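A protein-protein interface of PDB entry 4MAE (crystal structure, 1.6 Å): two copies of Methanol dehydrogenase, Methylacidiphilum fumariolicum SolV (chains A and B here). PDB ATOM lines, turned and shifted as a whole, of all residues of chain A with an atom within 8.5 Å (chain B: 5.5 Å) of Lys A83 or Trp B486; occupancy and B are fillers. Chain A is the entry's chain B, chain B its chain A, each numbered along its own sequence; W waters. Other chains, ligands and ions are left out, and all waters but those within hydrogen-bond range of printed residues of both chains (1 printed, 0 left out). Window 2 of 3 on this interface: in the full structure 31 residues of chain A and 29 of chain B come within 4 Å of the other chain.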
ATOM      1  N   ALA A  43       9.714 -16.194  -1.207  1.00  0.00           N
ATOM      2  CA  ALA A  43       9.037 -14.899  -1.368  1.00  0.00           C
ATOM      3  C   ALA A  43       9.961 -13.877  -2.013  1.00  0.00           C
ATOM      4  O   ALA A  43       9.572 -13.178  -2.947  1.00  0.00           O
ATOM      5  CB  ALA A  43       8.552 -14.389  -0.012  1.00  0.00           C
ATOM      6  N   TRP A  44      11.182 -13.778  -1.494  1.00  0.00           N
ATOM      7  CA  TRP A  44      12.191 -12.880  -2.038  1.00  0.00           C
ATOM      8  C   TRP A  44      13.568 -13.279  -1.538  1.00  0.00           C
ATOM      9  O   TRP A  44      13.685 -14.095  -0.626  1.00  0.00           O
ATOM     10  CB  TRP A  44      11.906 -11.425  -1.653  1.00  0.00           C
ATOM     11  CG  TRP A  44      11.736 -11.107  -0.171  1.00  0.00           C
ATOM     12  CD1 TRP A  44      10.568 -11.099   0.533  1.00  0.00           C
ATOM     13  CD2 TRP A  44      12.750 -10.656   0.740  1.00  0.00           C
ATOM     14  NE1 TRP A  44      10.795 -10.712   1.834  1.00  0.00           N
ATOM     15  CE2 TRP A  44      12.124 -10.425   1.984  1.00  0.00           C
ATOM     16  CE3 TRP A  44      14.129 -10.442   0.631  1.00  0.00           C
ATOM     17  CZ2 TRP A  44      12.828  -9.985   3.104  1.00  0.00           C
ATOM     18  CZ3 TRP A  44      14.823 -10.005   1.734  1.00  0.00           C
ATOM     19  CH2 TRP A  44      14.178  -9.777   2.955  1.00  0.00           C
ATOM     20  N   ASP A  79      14.349  -1.930   4.276  1.00  0.00           N
ATOM     21  CA  ASP A  79      13.015  -1.426   4.601  1.00  0.00           C
ATOM     22  C   ASP A  79      11.971  -2.397   4.063  1.00  0.00           C
ATOM     23  O   ASP A  79      11.731  -2.438   2.862  1.00  0.00           O
ATOM     24  CB  ASP A  79      12.836  -0.032   3.985  1.00  0.00           C
ATOM     25  CG  ASP A  79      11.495   0.605   4.314  1.00  0.00           C
ATOM     26  OD1 ASP A  79      10.599  -0.081   4.860  1.00  0.00           O
ATOM     27  OD2 ASP A  79      11.348   1.811   4.006  1.00  0.00           O
ATOM     28  N   LEU A  80      11.335  -3.151   4.960  1.00  0.00           N
ATOM     29  CA  LEU A  80      10.377  -4.194   4.580  1.00  0.00           C
ATOM     30  C   LEU A  80       9.006  -3.654   4.170  1.00  0.00           C
ATOM     31  O   LEU A  80       8.131  -4.440   3.798  1.00  0.00           O
ATOM     32  CB  LEU A  80      10.214  -5.210   5.720  1.00  0.00           C
ATOM     33  CG  LEU A  80      11.492  -5.911   6.186  1.00  0.00           C
ATOM     34  CD1 LEU A  80      11.186  -6.866   7.353  1.00  0.00           C
ATOM     35  CD2 LEU A  80      12.155  -6.664   5.023  1.00  0.00           C
ATOM     36  N   THR A  81       8.816  -2.332   4.222  1.00  0.00           N
ATOM     37  CA  THR A  81       7.572  -1.725   3.729  1.00  0.00           C
ATOM     38  C   THR A  81       7.563  -1.526   2.217  1.00  0.00           C
ATOM     39  O   THR A  81       6.533  -1.165   1.668  1.00  0.00           O
ATOM     40  CB  THR A  81       7.248  -0.356   4.413  1.00  0.00           C
ATOM     41  OG1 THR A  81       8.223   0.645   4.048  1.00  0.00           O
ATOM     42  CG2 THR A  81       7.175  -0.506   5.923  1.00  0.00           C
ATOM     43  N   GLN A  82       8.692  -1.781   1.547  1.00  0.00           N
ATOM     44  CA  GLN A  82       8.876  -1.390   0.141  1.00  0.00           C
ATOM     45  C   GLN A  82       8.674  -2.508  -0.887  1.00  0.00           C
ATOM     46  O   GLN A  82       9.191  -2.431  -2.014  1.00  0.00           O
ATOM     47  CB  GLN A  82      10.256  -0.753  -0.016  1.00  0.00           C
ATOM     48  CG  GLN A  82      10.425   0.477   0.847  1.00  0.00           C
ATOM     49  CD  GLN A  82       9.418   1.552   0.502  1.00  0.00           C
ATOM     50  OE1 GLN A  82       9.294   1.945  -0.659  1.00  0.00           O
ATOM     51  NE2 GLN A  82       8.682   2.028   1.504  1.00  0.00           N
ATOM     52  N   LYS A  83       7.901  -3.520  -0.500  1.00  0.00           N
ATOM     53  CA  LYS A  83       7.300  -4.488  -1.421  1.00  0.00           C
ATOM     54  C   LYS A  83       8.278  -5.151  -2.416  1.00  0.00           C
ATOM     55  O   LYS A  83       8.296  -4.806  -3.601  1.00  0.00           O
ATOM     56  CB  LYS A  83       6.138  -3.820  -2.170  1.00  0.00           C
ATOM     57  CG  LYS A  83       5.105  -3.169  -1.254  1.00  0.00           C
ATOM     58  CD  LYS A  83       3.910  -2.650  -2.043  1.00  0.00           C
ATOM     59  CE  LYS A  83       2.772  -2.222  -1.119  1.00  0.00           C
ATOM     60  NZ  LYS A  83       1.482  -2.021  -1.882  1.00  0.00           N
ATOM     61  N   PRO A  84       9.069  -6.131  -1.948  1.00  0.00           N
ATOM     62  CA  PRO A  84       9.150  -6.654  -0.578  1.00  0.00           C
ATOM     63  C   PRO A  84      10.150  -5.926   0.327  1.00  0.00           C
ATOM     64  O   PRO A  84      10.018  -5.960   1.553  1.00  0.00           O
ATOM     65  CB  PRO A  84       9.590  -8.106  -0.799  1.00  0.00           C
ATOM     66  CG  PRO A  84      10.408  -8.065  -2.039  1.00  0.00           C
ATOM     67  CD  PRO A  84       9.874  -6.942  -2.886  1.00  0.00           C
ATOM     68  N   TYR A  85      11.165  -5.309  -0.270  1.00  0.00           N
ATOM     69  CA  TYR A  85      12.144  -4.541   0.482  1.00  0.00           C
ATOM     70  C   TYR A  85      12.840  -3.515  -0.395  1.00  0.00           C
ATOM     71  O   TYR A  85      12.802  -3.605  -1.620  1.00  0.00           O
ATOM     72  CB  TYR A  85      13.202  -5.467   1.108  1.00  0.00           C
ATOM     73  CG  TYR A  85      14.127  -6.138   0.108  1.00  0.00           C
ATOM     74  CD1 TYR A  85      13.813  -7.376  -0.444  1.00  0.00           C
ATOM     75  CD2 TYR A  85      15.325  -5.539  -0.274  1.00  0.00           C
ATOM     76  CE1 TYR A  85      14.655  -7.991  -1.357  1.00  0.00           C
ATOM     77  CE2 TYR A  85      16.173  -6.144  -1.189  1.00  0.00           C
ATOM     78  CZ  TYR A  85      15.835  -7.379  -1.723  1.00  0.00           C
ATOM     79  OH  TYR A  85      16.674  -7.989  -2.636  1.00  0.00           O
ATOM     80  N   ALA A  86      13.484  -2.550   0.250  1.00  0.00           N
ATOM     81  CA  ALA A  86      14.463  -1.690  -0.407  1.00  0.00           C
ATOM     82  C   ALA A  86      15.651  -1.538   0.531  1.00  0.00           C
ATOM     83  O   ALA A  86      15.508  -1.676   1.748  1.00  0.00           O
ATOM     84  CB  ALA A  86      13.858  -0.336  -0.739  1.00  0.00           C
ATOM     85  N   PRO A 517       5.502  -6.145   7.679  1.00  0.00           N
ATOM     86  CA  PRO A 517       4.476  -5.099   7.811  1.00  0.00           C
ATOM     87  C   PRO A 517       3.125  -5.471   7.192  1.00  0.00           C
ATOM     88  O   PRO A 517       2.115  -4.842   7.511  1.00  0.00           O
ATOM     89  CB  PRO A 517       5.081  -3.910   7.059  1.00  0.00           C
ATOM     90  CG  PRO A 517       6.544  -4.146   7.068  1.00  0.00           C
ATOM     91  CD  PRO A 517       6.743  -5.630   7.073  1.00  0.00           C
ATOM     92  N   ASP A 518       3.123  -6.457   6.295  1.00  0.00           N
ATOM     93  CA  ASP A 518       1.899  -7.016   5.718  1.00  0.00           C
ATOM     94  C   ASP A 518       1.187  -8.021   6.644  1.00  0.00           C
ATOM     95  O   ASP A 518       0.197  -8.634   6.240  1.00  0.00           O
ATOM     96  CB  ASP A 518       2.209  -7.677   4.365  1.00  0.00           C
ATOM     97  CG  ASP A 518       3.285  -8.765   4.459  1.00  0.00           C
ATOM     98  OD1 ASP A 518       3.818  -8.995   5.567  1.00  0.00           O
ATOM     99  OD2 ASP A 518       3.594  -9.380   3.420  1.00  0.00           O
ATOM    100  N   TYR A 522       7.081 -14.773   7.717  1.00  0.00           N
ATOM    101  CA  TYR A 522       8.193 -15.125   6.838  1.00  0.00           C
ATOM    102  C   TYR A 522       9.228 -15.947   7.590  1.00  0.00           C
ATOM    103  O   TYR A 522       9.383 -15.801   8.805  1.00  0.00           O
ATOM    104  CB  TYR A 522       8.866 -13.860   6.312  1.00  0.00           C
ATOM    105  CG  TYR A 522       7.991 -13.074   5.386  1.00  0.00           C
ATOM    106  CD1 TYR A 522       7.123 -12.104   5.885  1.00  0.00           C
ATOM    107  CD2 TYR A 522       8.004 -13.316   4.013  1.00  0.00           C
ATOM    108  CE1 TYR A 522       6.296 -11.394   5.043  1.00  0.00           C
ATOM    109  CE2 TYR A 522       7.179 -12.608   3.163  1.00  0.00           C
ATOM    110  CZ  TYR A 522       6.333 -11.645   3.680  1.00  0.00           C
ATOM    111  OH  TYR A 522       5.509 -10.936   2.835  1.00  0.00           O
ATOM    112  N   TYR B 480      11.998 -11.661 -18.654  1.00  0.00           N
ATOM    113  CA  TYR B 480      13.222 -10.861 -18.603  1.00  0.00           C
ATOM    114  C   TYR B 480      13.460 -10.361 -17.194  1.00  0.00           C
ATOM    115  O   TYR B 480      12.544 -10.346 -16.373  1.00  0.00           O
ATOM    116  CB  TYR B 480      13.176  -9.670 -19.576  1.00  0.00           C
ATOM    117  CG  TYR B 480      12.226  -8.549 -19.206  1.00  0.00           C
ATOM    118  CD1 TYR B 480      12.674  -7.414 -18.540  1.00  0.00           C
ATOM    119  CD2 TYR B 480      10.868  -8.615 -19.543  1.00  0.00           C
ATOM    120  CE1 TYR B 480      11.800  -6.365 -18.217  1.00  0.00           C
ATOM    121  CE2 TYR B 480       9.989  -7.583 -19.225  1.00  0.00           C
ATOM    122  CZ  TYR B 480      10.456  -6.464 -18.557  1.00  0.00           C
ATOM    123  OH  TYR B 480       9.584  -5.441 -18.250  1.00  0.00           O
ATOM    124  N   GLY B 481      14.700  -9.957 -16.922  1.00  0.00           N
ATOM    125  CA  GLY B 481      15.085  -9.434 -15.616  1.00  0.00           C
ATOM    126  C   GLY B 481      15.411  -7.949 -15.636  1.00  0.00           C
ATOM    127  O   GLY B 481      15.731  -7.383 -16.688  1.00  0.00           O
ATOM    128  N   THR B 482      15.333  -7.321 -14.463  1.00  0.00           N
ATOM    129  CA  THR B 482      15.678  -5.909 -14.302  1.00  0.00           C
ATOM    130  C   THR B 482      16.949  -5.769 -13.476  1.00  0.00           C
ATOM    131  O   THR B 482      17.323  -6.674 -12.724  1.00  0.00           O
ATOM    132  CB  THR B 482      14.564  -5.090 -13.607  1.00  0.00           C
ATOM    133  OG1 THR B 482      14.471  -5.460 -12.220  1.00  0.00           O
ATOM    134  CG2 THR B 482      13.224  -5.284 -14.284  1.00  0.00           C
ATOM    135  N   ASP B 484      17.524  -4.032 -10.901  1.00  0.00           N
ATOM    136  CA  ASP B 484      17.312  -4.060  -9.459  1.00  0.00           C
ATOM    137  C   ASP B 484      16.693  -5.364  -8.956  1.00  0.00           C
ATOM    138  O   ASP B 484      16.179  -5.418  -7.840  1.00  0.00           O
ATOM    139  CB  ASP B 484      16.534  -2.833  -8.983  1.00  0.00           C
ATOM    140  CG  ASP B 484      15.123  -2.770  -9.510  1.00  0.00           C
ATOM    141  OD1 ASP B 484      14.800  -3.401 -10.543  1.00  0.00           O
ATOM    142  OD2 ASP B 484      14.321  -2.047  -8.877  1.00  0.00           O
ATOM    143  N   GLY B 485      16.779  -6.419  -9.765  1.00  0.00           N
ATOM    144  CA  GLY B 485      16.588  -7.785  -9.272  1.00  0.00           C
ATOM    145  C   GLY B 485      15.234  -8.419  -9.505  1.00  0.00           C
ATOM    146  O   GLY B 485      14.997  -9.542  -9.068  1.00  0.00           O
ATOM    147  N   TRP B 486      14.347  -7.733 -10.209  1.00  0.00           N
ATOM    148  CA  TRP B 486      13.039  -8.306 -10.506  1.00  0.00           C
ATOM    149  C   TRP B 486      13.102  -9.186 -11.740  1.00  0.00           C
ATOM    150  O   TRP B 486      13.538  -8.732 -12.807  1.00  0.00           O
ATOM    151  CB  TRP B 486      12.001  -7.213 -10.725  1.00  0.00           C
ATOM    152  CG  TRP B 486      11.633  -6.520  -9.482  1.00  0.00           C
ATOM    153  CD1 TRP B 486      12.162  -5.358  -8.997  1.00  0.00           C
ATOM    154  CD2 TRP B 486      10.648  -6.940  -8.541  1.00  0.00           C
ATOM    155  NE1 TRP B 486      11.558  -5.028  -7.803  1.00  0.00           N
ATOM    156  CE2 TRP B 486      10.627  -5.988  -7.502  1.00  0.00           C
ATOM    157  CE3 TRP B 486       9.774  -8.034  -8.475  1.00  0.00           C
ATOM    158  CZ2 TRP B 486       9.761  -6.091  -6.414  1.00  0.00           C
ATOM    159  CZ3 TRP B 486       8.927  -8.144  -7.385  1.00  0.00           C
ATOM    160  CH2 TRP B 486       8.922  -7.173  -6.377  1.00  0.00           C
ATOM    161  N   PHE B 487      12.648 -10.430 -11.590  1.00  0.00           N
ATOM    162  CA  PHE B 487      12.459 -11.332 -12.718  1.00  0.00           C
ATOM    163  C   PHE B 487      10.969 -11.306 -13.053  1.00  0.00           C
ATOM    164  O   PHE B 487      10.125 -11.455 -12.164  1.00  0.00           O
ATOM    165  CB  PHE B 487      12.943 -12.745 -12.378  1.00  0.00           C
ATOM    166  CG  PHE B 487      13.026 -13.680 -13.567  1.00  0.00           C
ATOM    167  CD1 PHE B 487      13.573 -13.263 -14.775  1.00  0.00           C
ATOM    168  CD2 PHE B 487      12.584 -14.996 -13.462  1.00  0.00           C
ATOM    169  CE1 PHE B 487      13.649 -14.123 -15.866  1.00  0.00           C
ATOM    170  CE2 PHE B 487      12.663 -15.868 -14.550  1.00  0.00           C
ATOM    171  CZ  PHE B 487      13.201 -15.432 -15.752  1.00  0.00           C
ATOM    172  N   LYS B 488      10.650 -11.072 -14.325  1.00  0.00           N
ATOM    173  CA  LYS B 488       9.283 -10.782 -14.725  1.00  0.00           C
ATOM    174  C   LYS B 488       8.849 -11.648 -15.884  1.00  0.00           C
ATOM    175  O   LYS B 488       9.659 -12.001 -16.740  1.00  0.00           O
ATOM    176  CB  LYS B 488       9.155  -9.318 -15.162  1.00  0.00           C
ATOM    177  CG  LYS B 488       9.530  -8.303 -14.119  1.00  0.00           C
ATOM    178  CD  LYS B 488       9.318  -6.886 -14.662  1.00  0.00           C
ATOM    179  CE  LYS B 488       9.574  -5.833 -13.601  1.00  0.00           C
ATOM    180  NZ  LYS B 488       9.143  -4.483 -14.063  1.00  0.00           N
ATOM    181  N   GLN B 500       5.992 -11.651 -11.173  1.00  0.00           N
ATOM    182  CA  GLN B 500       7.321 -11.110 -10.907  1.00  0.00           C
ATOM    183  C   GLN B 500       7.791 -11.497  -9.516  1.00  0.00           C
ATOM    184  O   GLN B 500       6.977 -11.725  -8.622  1.00  0.00           O
ATOM    185  CB  GLN B 500       7.371  -9.588 -11.098  1.00  0.00           C
ATOM    186  CG  GLN B 500       6.496  -8.781 -10.146  1.00  0.00           C
ATOM    187  CD  GLN B 500       6.578  -7.274 -10.370  1.00  0.00           C
ATOM    188  OE1 GLN B 500       6.938  -6.807 -11.450  1.00  0.00           O
ATOM    189  NE2 GLN B 500       6.242  -6.510  -9.339  1.00  0.00           N
ATOM    190  N   GLN B 501       9.111 -11.571  -9.356  1.00  0.00           N
ATOM    191  CA  GLN B 501       9.728 -11.921  -8.081  1.00  0.00           C
ATOM    192  C   GLN B 501      11.060 -11.198  -7.948  1.00  0.00           C
ATOM    193  O   GLN B 501      11.823 -11.101  -8.926  1.00  0.00           O
ATOM    194  CB  GLN B 501       9.933 -13.438  -7.981  1.00  0.00           C
ATOM    195  CG  GLN B 501      10.417 -13.903  -6.615  1.00  0.00           C
ATOM    196  CD  GLN B 501      10.358 -15.409  -6.422  1.00  0.00           C
ATOM    197  OE1 GLN B 501       9.418 -16.088  -6.870  1.00  0.00           O
ATOM    198  NE2 GLN B 501      11.358 -15.942  -5.722  1.00  0.00           N
ATOM    199  N   LYS B 502      11.338 -10.697  -6.744  1.00  0.00           N
ATOM    200  CA  LYS B 502      12.579  -9.976  -6.482  1.00  0.00           C
ATOM    201  C   LYS B 502      13.657 -10.958  -6.027  1.00  0.00           C
ATOM    202  O   LYS B 502      13.498 -11.653  -5.013  1.00  0.00           O
ATOM    203  CB  LYS B 502      12.399  -8.856  -5.452  1.00  0.00           C
ATOM    204  CG  LYS B 502      13.583  -7.858  -5.486  1.00  0.00           C
ATOM    205  CD  LYS B 502      13.385  -6.617  -4.652  1.00  0.00           C
ATOM    206  CE  LYS B 502      14.625  -5.716  -4.722  1.00  0.00           C
ATOM    207  NZ  LYS B 502      14.457  -4.395  -4.028  1.00  0.00           N
ATOM    208  N   LEU B 503      14.726 -11.019  -6.813  1.00  0.00           N
ATOM    209  CA  LEU B 503      15.852 -11.903  -6.577  1.00  0.00           C
ATOM    210  C   LEU B 503      16.984 -11.118  -5.901  1.00  0.00           C
ATOM    211  O   LEU B 503      16.862  -9.915  -5.636  1.00  0.00           O
ATOM    212  CB  LEU B 503      16.323 -12.520  -7.900  1.00  0.00           C
ATOM    213  CG  LEU B 503      15.262 -13.220  -8.752  1.00  0.00           C
ATOM    214  CD1 LEU B 503      15.934 -13.954  -9.925  1.00  0.00           C
ATOM    215  CD2 LEU B 503      14.435 -14.163  -7.899  1.00  0.00           C
ATOM    216  N   ILE B 507      19.661  -8.469 -12.374  1.00  0.00           N
ATOM    217  CA  ILE B 507      19.713  -9.514 -13.382  1.00  0.00           C
ATOM    218  C   ILE B 507      20.250  -8.943 -14.694  1.00  0.00           C
ATOM    219  O   ILE B 507      19.623  -8.070 -15.304  1.00  0.00           O
ATOM    220  CB  ILE B 507      18.302 -10.100 -13.605  1.00  0.00           C
ATOM    221  CG1 ILE B 507      17.779 -10.761 -12.320  1.00  0.00           C
ATOM    222  CG2 ILE B 507      18.300 -11.118 -14.775  1.00  0.00           C
ATOM    223  CD1 ILE B 507      16.274 -10.960 -12.313  1.00  0.00           C
HETATM  224  O   HOH W   1       9.489 -10.875  -4.534  1.00  0.00           O
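The side-chain amino group (NZ) of Lys B502 is in hydrogen-bond range of the backbone carbonyl oxygen (O) of Tyr A85, at 3.0 Å.
The backbone NH (N) of Trp B486 lies within hydrogen-bond range of the side-chain hydroxyl (OG1) of Thr B482 (3.0 Å).
The backbone NH of Leu B503 sits at hydrogen-bond distance from the backbone carbonyl oxygen of Gly B485 (2.7 Å).
O of Gln B501 lies within hydrogen-bond range of N of Phe B487.
Among the printed residues, pairs that only touch across the chains: Ala A43 with Gln B501 (3.8 Å), Trp A44 with Lys B502 (3.5 Å), Lys A83 with Trp B486 (3.4 Å), Pro A84 with Trp B486 (3.6 Å), Pro A84 with Lys B502 (3.9 Å) and Tyr A85 with Leu B503 (3.6 Å).
Of the printed residues of chain B, Ala A43 touches Gln B501 (3.8 Å).
Printed residues of chain B within 4 Å of Trp A44: Lys B502.
Lys A83 touches just one residue of chain B: Trp B486.
Of the printed residues of chain B, Pro A84 touches Trp B486 (3.6 Å) and Lys B502 (3.9 Å).
No residue of chain A comes within 4 Å of Gly B485.
Trp B486 touches just these residues of chain A: Lys A83 (3.4 Å) and Pro A84 (3.6 Å).
Of the printed residues of chain A, Leu B503 touches Tyr A85 (3.6 Å).
The nearest printed residue of chain B that does not touch Lys A83 is Lys B502 (5.5 Å).
The nearest residue of chain A that does not touch Trp B486 is Gln A82 (5.8 Å).
The nearest printed residue of chain B that does not touch Tyr A85 is Asp B484 (5.8 Å).
Of the 13 printed residues of chain B, 4 touch a printed residue of chain A.
Printed residues of chain B that touch a printed residue of chain A: Trp B486, Gln B501, Lys B502 and Leu B503.
Hydrophobic or aromatic side chains of chain B that line the printed part of chain A: Trp B486.
Among the printed residues, 7 pairs touch across the chains.
No position is printed for both chains.
Of the 7 pairs that touch across the chains among the printed residues, none has its exchanged pair printed and touching as well.
Water W1 lies within hydrogen-bond range of the backbone carbonyl oxygen of Ala A43 (2.8 Å) and the backbone NH of Lys B502 (2.9 Å).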
